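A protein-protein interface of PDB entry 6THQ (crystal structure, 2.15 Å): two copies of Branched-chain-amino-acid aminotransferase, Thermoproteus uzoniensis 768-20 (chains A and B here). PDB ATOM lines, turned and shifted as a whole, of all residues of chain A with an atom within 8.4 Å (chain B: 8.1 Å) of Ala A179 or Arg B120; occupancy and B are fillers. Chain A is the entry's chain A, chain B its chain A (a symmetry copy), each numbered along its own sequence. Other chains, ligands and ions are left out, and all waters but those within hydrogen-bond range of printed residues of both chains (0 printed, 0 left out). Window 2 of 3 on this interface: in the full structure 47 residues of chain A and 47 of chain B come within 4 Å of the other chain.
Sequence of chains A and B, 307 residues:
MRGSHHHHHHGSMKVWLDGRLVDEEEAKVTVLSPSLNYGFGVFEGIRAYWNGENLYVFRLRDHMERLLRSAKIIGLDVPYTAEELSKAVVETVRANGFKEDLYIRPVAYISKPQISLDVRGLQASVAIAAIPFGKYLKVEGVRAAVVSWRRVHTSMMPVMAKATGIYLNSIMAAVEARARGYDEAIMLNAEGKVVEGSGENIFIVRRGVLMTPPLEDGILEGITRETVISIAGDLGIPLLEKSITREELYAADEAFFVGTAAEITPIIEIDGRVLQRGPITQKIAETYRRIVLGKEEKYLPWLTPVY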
ATOM      1  N   ILE A 171     -24.459  10.394  14.359  1.00  0.00           N
ATOM      2  CA  ILE A 171     -23.947   9.995  13.041  1.00  0.00           C
ATOM      3  C   ILE A 171     -22.536  10.474  12.744  1.00  0.00           C
ATOM      4  O   ILE A 171     -21.690   9.658  12.351  1.00  0.00           O
ATOM      5  CB  ILE A 171     -24.929  10.317  11.926  1.00  0.00           C
ATOM      6  CG1 ILE A 171     -26.048   9.282  12.024  1.00  0.00           C
ATOM      7  CG2 ILE A 171     -24.238  10.141  10.591  1.00  0.00           C
ATOM      8  CD1 ILE A 171     -27.268   9.633  11.212  1.00  0.00           C
ATOM      9  N   MET A 172     -22.263  11.772  12.935  1.00  0.00           N
ATOM     10  CA  MET A 172     -20.906  12.280  12.642  1.00  0.00           C
ATOM     11  C   MET A 172     -19.916  11.437  13.485  1.00  0.00           C
ATOM     12  O   MET A 172     -18.882  10.993  12.995  1.00  0.00           O
ATOM     13  CB  MET A 172     -20.763  13.751  13.070  1.00  0.00           C
ATOM     14  CG  MET A 172     -21.704  14.781  12.421  1.00  0.00           C
ATOM     15  SD  MET A 172     -21.434  15.022  10.647  1.00  0.00           S
ATOM     16  CE  MET A 172     -22.627  13.852  10.115  1.00  0.00           C
ATOM     17  N   ALA A 173     -20.231  11.217  14.772  1.00  0.00           N
ATOM     18  CA  ALA A 173     -19.339  10.494  15.651  1.00  0.00           C
ATOM     19  C   ALA A 173     -19.104   9.052  15.169  1.00  0.00           C
ATOM     20  O   ALA A 173     -17.943   8.568  15.087  1.00  0.00           O
ATOM     21  CB  ALA A 173     -19.866  10.506  17.101  1.00  0.00           C
ATOM     22  N   ALA A 174     -20.193   8.369  14.891  1.00  0.00           N
ATOM     23  CA  ALA A 174     -20.151   6.922  14.532  1.00  0.00           C
ATOM     24  C   ALA A 174     -19.398   6.734  13.217  1.00  0.00           C
ATOM     25  O   ALA A 174     -18.494   5.904  13.124  1.00  0.00           O
ATOM     26  CB  ALA A 174     -21.580   6.416  14.389  1.00  0.00           C
ATOM     27  N   VAL A 175     -19.700   7.580  12.237  1.00  0.00           N
ATOM     28  CA  VAL A 175     -19.015   7.505  10.966  1.00  0.00           C
ATOM     29  C   VAL A 175     -17.535   7.782  11.125  1.00  0.00           C
ATOM     30  O   VAL A 175     -16.691   7.025  10.627  1.00  0.00           O
ATOM     31  CB  VAL A 175     -19.684   8.431   9.909  1.00  0.00           C
ATOM     32  CG1 VAL A 175     -18.845   8.557   8.618  1.00  0.00           C
ATOM     33  CG2 VAL A 175     -21.071   7.875   9.576  1.00  0.00           C
ATOM     34  N   GLU A 176     -17.187   8.806  11.868  1.00  0.00           N
ATOM     35  CA  GLU A 176     -15.772   9.069  12.037  1.00  0.00           C
ATOM     36  C   GLU A 176     -15.016   7.882  12.651  1.00  0.00           C
ATOM     37  O   GLU A 176     -13.930   7.530  12.194  1.00  0.00           O
ATOM     38  CB  GLU A 176     -15.519  10.367  12.839  1.00  0.00           C
ATOM     39  CG  GLU A 176     -14.068  10.542  13.294  1.00  0.00           C
ATOM     40  CD  GLU A 176     -13.826  11.820  14.136  1.00  0.00           C
ATOM     41  OE1 GLU A 176     -12.844  11.825  14.906  1.00  0.00           O
ATOM     42  OE2 GLU A 176     -14.593  12.826  14.025  1.00  0.00           O
ATOM     43  N   ALA A 177     -15.563   7.246  13.680  1.00  0.00           N
ATOM     44  CA  ALA A 177     -14.804   6.146  14.280  1.00  0.00           C
ATOM     45  C   ALA A 177     -14.693   4.963  13.315  1.00  0.00           C
ATOM     46  O   ALA A 177     -13.630   4.355  13.169  1.00  0.00           O
ATOM     47  CB  ALA A 177     -15.482   5.697  15.565  1.00  0.00           C
ATOM     48  N   ARG A 178     -15.814   4.624  12.685  1.00  0.00           N
ATOM     49  CA  ARG A 178     -15.883   3.471  11.765  1.00  0.00           C
ATOM     50  C   ARG A 178     -14.940   3.697  10.549  1.00  0.00           C
ATOM     51  O   ARG A 178     -14.141   2.824  10.221  1.00  0.00           O
ATOM     52  CB  ARG A 178     -17.345   3.117  11.430  1.00  0.00           C
ATOM     53  CG  ARG A 178     -18.064   2.286  12.524  1.00  0.00           C
ATOM     54  CD  ARG A 178     -19.617   2.366  12.417  1.00  0.00           C
ATOM     55  NE  ARG A 178     -20.390   1.668  13.504  1.00  0.00           N
ATOM     56  CZ  ARG A 178     -20.655   2.149  14.738  1.00  0.00           C
ATOM     57  NH1 ARG A 178     -20.200   3.336  15.099  1.00  0.00           N
ATOM     58  NH2 ARG A 178     -21.301   1.420  15.655  1.00  0.00           N
ATOM     59  N   ALA A 179     -14.921   4.903   9.989  1.00  0.00           N
ATOM     60  CA  ALA A 179     -14.048   5.183   8.837  1.00  0.00           C
ATOM     61  C   ALA A 179     -12.599   4.972   9.209  1.00  0.00           C
ATOM     62  O   ALA A 179     -11.801   4.540   8.386  1.00  0.00           O
ATOM     63  CB  ALA A 179     -14.268   6.622   8.259  1.00  0.00           C
ATOM     64  N   ARG A 180     -12.245   5.245  10.457  1.00  0.00           N
ATOM     65  CA  ARG A 180     -10.839   5.177  10.876  1.00  0.00           C
ATOM     66  C   ARG A 180     -10.503   3.721  11.323  1.00  0.00           C
ATOM     67  O   ARG A 180      -9.451   3.502  11.912  1.00  0.00           O
ATOM     68  CB  ARG A 180     -10.549   6.210  11.985  1.00  0.00           C
ATOM     69  CG  ARG A 180     -10.864   7.705  11.662  1.00  0.00           C
ATOM     70  CD  ARG A 180     -10.674   8.746  12.840  1.00  0.00           C
ATOM     71  NE  ARG A 180     -10.910  10.157  12.397  1.00  0.00           N
ATOM     72  CZ  ARG A 180     -10.457  11.334  12.909  1.00  0.00           C
ATOM     73  NH1 ARG A 180      -9.585  11.383  13.973  1.00  0.00           N
ATOM     74  NH2 ARG A 180     -10.889  12.510  12.281  1.00  0.00           N
ATOM     75  N   GLY A 181     -11.373   2.736  11.029  1.00  0.00           N
ATOM     76  CA  GLY A 181     -11.166   1.335  11.400  1.00  0.00           C
ATOM     77  C   GLY A 181     -11.709   0.826  12.785  1.00  0.00           C
ATOM     78  O   GLY A 181     -11.624  -0.386  13.088  1.00  0.00           O
ATOM     79  N   TYR A 182     -12.268   1.701  13.636  1.00  0.00           N
ATOM     80  CA  TYR A 182     -12.734   1.268  14.966  1.00  0.00           C
ATOM     81  C   TYR A 182     -14.199   0.821  14.987  1.00  0.00           C
ATOM     82  O   TYR A 182     -14.945   1.040  14.009  1.00  0.00           O
ATOM     83  CB  TYR A 182     -12.526   2.374  16.011  1.00  0.00           C
ATOM     84  CG  TYR A 182     -11.116   2.886  16.159  1.00  0.00           C
ATOM     85  CD1 TYR A 182     -10.555   3.796  15.222  1.00  0.00           C
ATOM     86  CD2 TYR A 182     -10.349   2.517  17.246  1.00  0.00           C
ATOM     87  CE1 TYR A 182      -9.240   4.284  15.380  1.00  0.00           C
ATOM     88  CE2 TYR A 182      -9.015   2.991  17.406  1.00  0.00           C
ATOM     89  CZ  TYR A 182      -8.478   3.871  16.492  1.00  0.00           C
ATOM     90  OH  TYR A 182      -7.216   4.343  16.699  1.00  0.00           O
ATOM     91  N   ASP A 183     -14.621   0.216  16.091  1.00  0.00           N
ATOM     92  CA  ASP A 183     -15.997  -0.275  16.198  1.00  0.00           C
ATOM     93  C   ASP A 183     -16.982   0.778  16.658  1.00  0.00           C
ATOM     94  O   ASP A 183     -18.184   0.729  16.290  1.00  0.00           O
ATOM     95  CB  ASP A 183     -16.068  -1.479  17.153  1.00  0.00           C
ATOM     96  CG  ASP A 183     -15.022  -2.564  16.806  1.00  0.00           C
ATOM     97  OD1 ASP A 183     -15.137  -3.152  15.729  1.00  0.00           O
ATOM     98  OD2 ASP A 183     -14.068  -2.785  17.580  1.00  0.00           O
ATOM     99  N   GLU A 184     -16.491   1.727  17.446  1.00  0.00           N
ATOM    100  CA  GLU A 184     -17.349   2.695  18.083  1.00  0.00           C
ATOM    101  C   GLU A 184     -16.615   3.988  18.510  1.00  0.00           C
ATOM    102  O   GLU A 184     -15.393   4.032  18.748  1.00  0.00           O
ATOM    103  CB  GLU A 184     -18.038   2.033  19.293  1.00  0.00           C
ATOM    104  CG  GLU A 184     -19.260   2.746  19.838  1.00  0.00           C
ATOM    105  CD  GLU A 184     -20.247   3.234  18.752  1.00  0.00           C
ATOM    106  OE1 GLU A 184     -20.047   4.370  18.173  1.00  0.00           O
ATOM    107  OE2 GLU A 184     -21.249   2.483  18.507  1.00  0.00           O
ATOM    108  N   PHE B  40     -30.668  12.912   9.396  1.00  0.00           N
ATOM    109  CA  PHE B  40     -29.566  12.855   8.435  1.00  0.00           C
ATOM    110  C   PHE B  40     -30.056  13.105   7.001  1.00  0.00           C
ATOM    111  O   PHE B  40     -30.318  12.184   6.259  1.00  0.00           O
ATOM    112  CB  PHE B  40     -28.846  11.524   8.572  1.00  0.00           C
ATOM    113  CG  PHE B  40     -27.684  11.381   7.658  1.00  0.00           C
ATOM    114  CD1 PHE B  40     -26.479  12.030   7.947  1.00  0.00           C
ATOM    115  CD2 PHE B  40     -27.753  10.550   6.489  1.00  0.00           C
ATOM    116  CE1 PHE B  40     -25.358  11.856   7.114  1.00  0.00           C
ATOM    117  CE2 PHE B  40     -26.628  10.380   5.692  1.00  0.00           C
ATOM    118  CZ  PHE B  40     -25.439  11.031   5.988  1.00  0.00           C
ATOM    119  N   GLY B  75     -21.593  14.277   4.828  1.00  0.00           N
ATOM    120  CA  GLY B  75     -21.291  12.921   4.336  1.00  0.00           C
ATOM    121  C   GLY B  75     -22.467  12.199   3.643  1.00  0.00           C
ATOM    122  O   GLY B  75     -22.542  10.979   3.685  1.00  0.00           O
ATOM    123  N   ASP B  77     -24.343  11.156   0.233  1.00  0.00           N
ATOM    124  CA  ASP B  77     -24.065  11.035  -1.180  1.00  0.00           C
ATOM    125  C   ASP B  77     -25.266  11.403  -2.039  1.00  0.00           C
ATOM    126  O   ASP B  77     -26.261  10.647  -2.048  1.00  0.00           O
ATOM    127  CB  ASP B  77     -23.581   9.634  -1.537  1.00  0.00           C
ATOM    128  CG  ASP B  77     -23.056   9.560  -2.967  1.00  0.00           C
ATOM    129  OD1 ASP B  77     -23.111  10.542  -3.767  1.00  0.00           O
ATOM    130  OD2 ASP B  77     -22.527   8.503  -3.302  1.00  0.00           O
ATOM    131  N   ILE B 110     -32.344   9.640   2.793  1.00  0.00           N
ATOM    132  CA  ILE B 110     -32.159   8.237   2.523  1.00  0.00           C
ATOM    133  C   ILE B 110     -33.514   7.512   2.485  1.00  0.00           C
ATOM    134  O   ILE B 110     -34.288   7.595   3.435  1.00  0.00           O
ATOM    135  CB  ILE B 110     -31.187   7.656   3.524  1.00  0.00           C
ATOM    136  CG1 ILE B 110     -29.815   8.144   3.012  1.00  0.00           C
ATOM    137  CG2 ILE B 110     -31.260   6.133   3.443  1.00  0.00           C
ATOM    138  CD1 ILE B 110     -28.746   7.978   4.035  1.00  0.00           C
ATOM    139  N   LYS B 112     -34.058   4.133   1.870  1.00  0.00           N
ATOM    140  CA  LYS B 112     -33.916   2.791   2.466  1.00  0.00           C
ATOM    141  C   LYS B 112     -34.254   2.784   4.003  1.00  0.00           C
ATOM    142  O   LYS B 112     -33.867   3.675   4.752  1.00  0.00           O
ATOM    143  CB  LYS B 112     -32.473   2.302   2.126  1.00  0.00           C
ATOM    144  CG  LYS B 112     -31.903   1.075   2.871  1.00  0.00           C
ATOM    145  CD  LYS B 112     -30.589   0.616   2.250  1.00  0.00           C
ATOM    146  CE  LYS B 112     -30.179  -0.794   2.666  1.00  0.00           C
ATOM    147  NZ  LYS B 112     -29.503  -0.674   3.982  1.00  0.00           N
ATOM    148  N   GLN B 114     -33.429   1.861   7.746  1.00  0.00           N
ATOM    149  CA  GLN B 114     -32.135   1.462   8.380  1.00  0.00           C
ATOM    150  C   GLN B 114     -32.021   2.014   9.774  1.00  0.00           C
ATOM    151  O   GLN B 114     -32.082   3.207   9.974  1.00  0.00           O
ATOM    152  CB  GLN B 114     -30.893   1.838   7.561  1.00  0.00           C
ATOM    153  CG  GLN B 114     -29.592   1.430   8.214  1.00  0.00           C
ATOM    154  CD  GLN B 114     -28.384   1.743   7.332  1.00  0.00           C
ATOM    155  OE1 GLN B 114     -28.356   1.385   6.167  1.00  0.00           O
ATOM    156  NE2 GLN B 114     -27.384   2.414   7.881  1.00  0.00           N
ATOM    157  N   SER B 116     -29.309   1.154  11.705  1.00  0.00           N
ATOM    158  CA  SER B 116     -27.857   1.399  11.963  1.00  0.00           C
ATOM    159  C   SER B 116     -27.442   2.870  11.708  1.00  0.00           C
ATOM    160  O   SER B 116     -27.917   3.512  10.759  1.00  0.00           O
ATOM    161  CB  SER B 116     -26.983   0.474  11.101  1.00  0.00           C
ATOM    162  OG  SER B 116     -25.636   0.679  11.497  1.00  0.00           O
ATOM    163  N   LEU B 117     -26.593   3.396  12.560  1.00  0.00           N
ATOM    164  CA  LEU B 117     -26.110   4.754  12.371  1.00  0.00           C
ATOM    165  C   LEU B 117     -25.042   4.794  11.324  1.00  0.00           C
ATOM    166  O   LEU B 117     -24.610   5.855  10.921  1.00  0.00           O
ATOM    167  CB  LEU B 117     -25.543   5.307  13.670  1.00  0.00           C
ATOM    168  CG  LEU B 117     -26.508   5.538  14.809  1.00  0.00           C
ATOM    169  CD1 LEU B 117     -25.641   6.005  15.952  1.00  0.00           C
ATOM    170  CD2 LEU B 117     -27.533   6.590  14.432  1.00  0.00           C
ATOM    171  N   ASP B 118     -24.592   3.633  10.877  1.00  0.00           N
ATOM    172  CA  ASP B 118     -23.547   3.584   9.890  1.00  0.00           C
ATOM    173  C   ASP B 118     -24.137   3.899   8.515  1.00  0.00           C
ATOM    174  O   ASP B 118     -24.599   3.015   7.801  1.00  0.00           O
ATOM    175  CB  ASP B 118     -22.813   2.241   9.890  1.00  0.00           C
ATOM    176  CG  ASP B 118     -21.535   2.286   9.065  1.00  0.00           C
ATOM    177  OD1 ASP B 118     -21.233   3.350   8.414  1.00  0.00           O
ATOM    178  OD2 ASP B 118     -20.801   1.267   9.144  1.00  0.00           O
ATOM    179  N   VAL B 119     -24.115   5.165   8.147  1.00  0.00           N
ATOM    180  CA  VAL B 119     -24.786   5.542   6.896  1.00  0.00           C
ATOM    181  C   VAL B 119     -23.869   5.602   5.681  1.00  0.00           C
ATOM    182  O   VAL B 119     -24.277   6.029   4.607  1.00  0.00           O
ATOM    183  CB  VAL B 119     -25.575   6.847   7.025  1.00  0.00           C
ATOM    184  CG1 VAL B 119     -26.708   6.665   8.026  1.00  0.00           C
ATOM    185  CG2 VAL B 119     -24.652   8.022   7.345  1.00  0.00           C
ATOM    186  N   ARG B 120     -22.616   5.186   5.874  1.00  0.00           N
ATOM    187  CA  ARG B 120     -21.650   5.108   4.772  1.00  0.00           C
ATOM    188  C   ARG B 120     -22.185   4.275   3.605  1.00  0.00           C
ATOM    189  O   ARG B 120     -22.838   3.233   3.838  1.00  0.00           O
ATOM    190  CB  ARG B 120     -20.316   4.518   5.260  1.00  0.00           C
ATOM    191  CG  ARG B 120     -19.528   5.525   6.097  1.00  0.00           C
ATOM    192  CD  ARG B 120     -18.269   4.948   6.728  1.00  0.00           C
ATOM    193  NE  ARG B 120     -18.581   3.679   7.390  1.00  0.00           N
ATOM    194  CZ  ARG B 120     -17.713   2.678   7.574  1.00  0.00           C
ATOM    195  NH1 ARG B 120     -16.469   2.819   7.163  1.00  0.00           N
ATOM    196  NH2 ARG B 120     -18.108   1.543   8.171  1.00  0.00           N
ATOM    197  N   GLY B 121     -21.903   4.743   2.378  1.00  0.00           N
ATOM    198  CA  GLY B 121     -22.265   4.054   1.138  1.00  0.00           C
ATOM    199  C   GLY B 121     -23.724   4.199   0.682  1.00  0.00           C
ATOM    200  O   GLY B 121     -24.111   3.678  -0.362  1.00  0.00           O
ATOM    201  N   LEU B 122     -24.561   4.883   1.466  1.00  0.00           N
ATOM    202  CA  LEU B 122     -25.949   5.071   1.063  1.00  0.00           C
ATOM    203  C   LEU B 122     -26.080   6.122  -0.017  1.00  0.00           C
ATOM    204  O   LEU B 122     -25.230   6.961  -0.234  1.00  0.00           O
ATOM    205  CB  LEU B 122     -26.879   5.355   2.233  1.00  0.00           C
ATOM    206  CG  LEU B 122     -26.869   4.236   3.278  1.00  0.00           C
ATOM    207  CD1 LEU B 122     -27.904   4.468   4.373  1.00  0.00           C
ATOM    208  CD2 LEU B 122     -27.097   2.874   2.627  1.00  0.00           C
ATOM    209  N   GLN B 123     -27.180   6.048  -0.713  1.00  0.00           N
ATOM    210  CA  GLN B 123     -27.397   6.914  -1.834  1.00  0.00           C
ATOM    211  C   GLN B 123     -28.611   7.755  -1.532  1.00  0.00           C
ATOM    212  O   GLN B 123     -29.673   7.188  -1.308  1.00  0.00           O
ATOM    213  CB  GLN B 123     -27.765   6.023  -2.986  1.00  0.00           C
ATOM    214  CG  GLN B 123     -26.620   5.397  -3.735  1.00  0.00           C
ATOM    215  CD  GLN B 123     -26.129   6.338  -4.800  1.00  0.00           C
ATOM    216  OE1 GLN B 123     -26.695   6.433  -5.929  1.00  0.00           O
ATOM    217  NE2 GLN B 123     -25.060   7.061  -4.453  1.00  0.00           N
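Of the 14 printed residues of chain A, 3 touch a printed residue of chain B.
Printed residues of chain A that touch a printed residue of chain B: Ile A171, Arg A178 and Ala A179.
Hydrophobic or aromatic side chains of chain A within 4 Å of the printed part of chain B: Ile A171.
Along chain A the printed residues that touch a printed residue of chain B span positions 171 to 179.
Hydrophobic or aromatic side chains of chain B that line the printed part of chain A: Phe B40, Leu B117 and Val B119.
Ile A171 touches Phe B40 (CD1 to CB, 3.6 Å).
Leu B117 touches Ile A171.
Ile A171 touches Val B119.
Arg A178 touches Asp B118 (CD to OD2, 3.6 Å).
CB of Arg A178 touches NH2 of Arg B120, 3.7 Å away.
Arg B120 touches Ala A179 (NH1 to CA, 3.8 Å).
Ala A179 touches just one residue of chain B: Arg B120 (3.8 Å).
Printed residues of chain A within 4 Å of Arg B120: Arg A178 and Ala A179.
Printed residues of chain A within 4 Å of Asp B118: Arg A178 (3.6 Å).
Printed residues of chain A within 4 Å of Phe B40: Ile A171.
Printed residues of chain B within 4 Å of Ile A171: Phe B40 (3.6 Å), Leu B117 (3.9 Å) and Val B119 (3.9 Å).
Of the printed residues of chain A, Leu B117 touches Ile A171 (3.9 Å).
Of the printed residues of chain B, Arg A178 touches Asp B118 and Arg B120.
Ile B110 touches none of the printed residues of chain A.
The nearest residue of chain B that does not touch Ala A179 is Asp B118 (6.7 Å).
The nearest printed residue of chain A that does not touch Arg B120 is Val A175 (4.002 Å).
The nearest printed residue of chain A that does not touch Val B119 is Val A175 (4.2 Å).
NH2 of Arg A178 sits close to O of Asp A183 (3.3 Å).
The guanidinium group (NH2) of Arg A178 lies within salt-bridge range of the side-chain carboxylate (OE2) of Glu A184, 3.0 Å away.
The side-chain amide nitrogen (NE2) of Gln B114 is in hydrogen-bond range of the backbone carbonyl oxygen (O) of Asp B118 (2.9 Å).
The side-chain hydroxyl (OG) of Ser B116 lies close to the backbone NH (N) of Asp B118, 3.2 Å away.
The side-chain carboxylate (OD1) of Asp B118 lies within salt-bridge range of the guanidinium group (NE) of Arg B120, 2.9 Å away.
No position is printed for both chains.
Of the 6 pairs that touch across the chains among the printed residues, none has its exchanged pair printed and touching as well.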
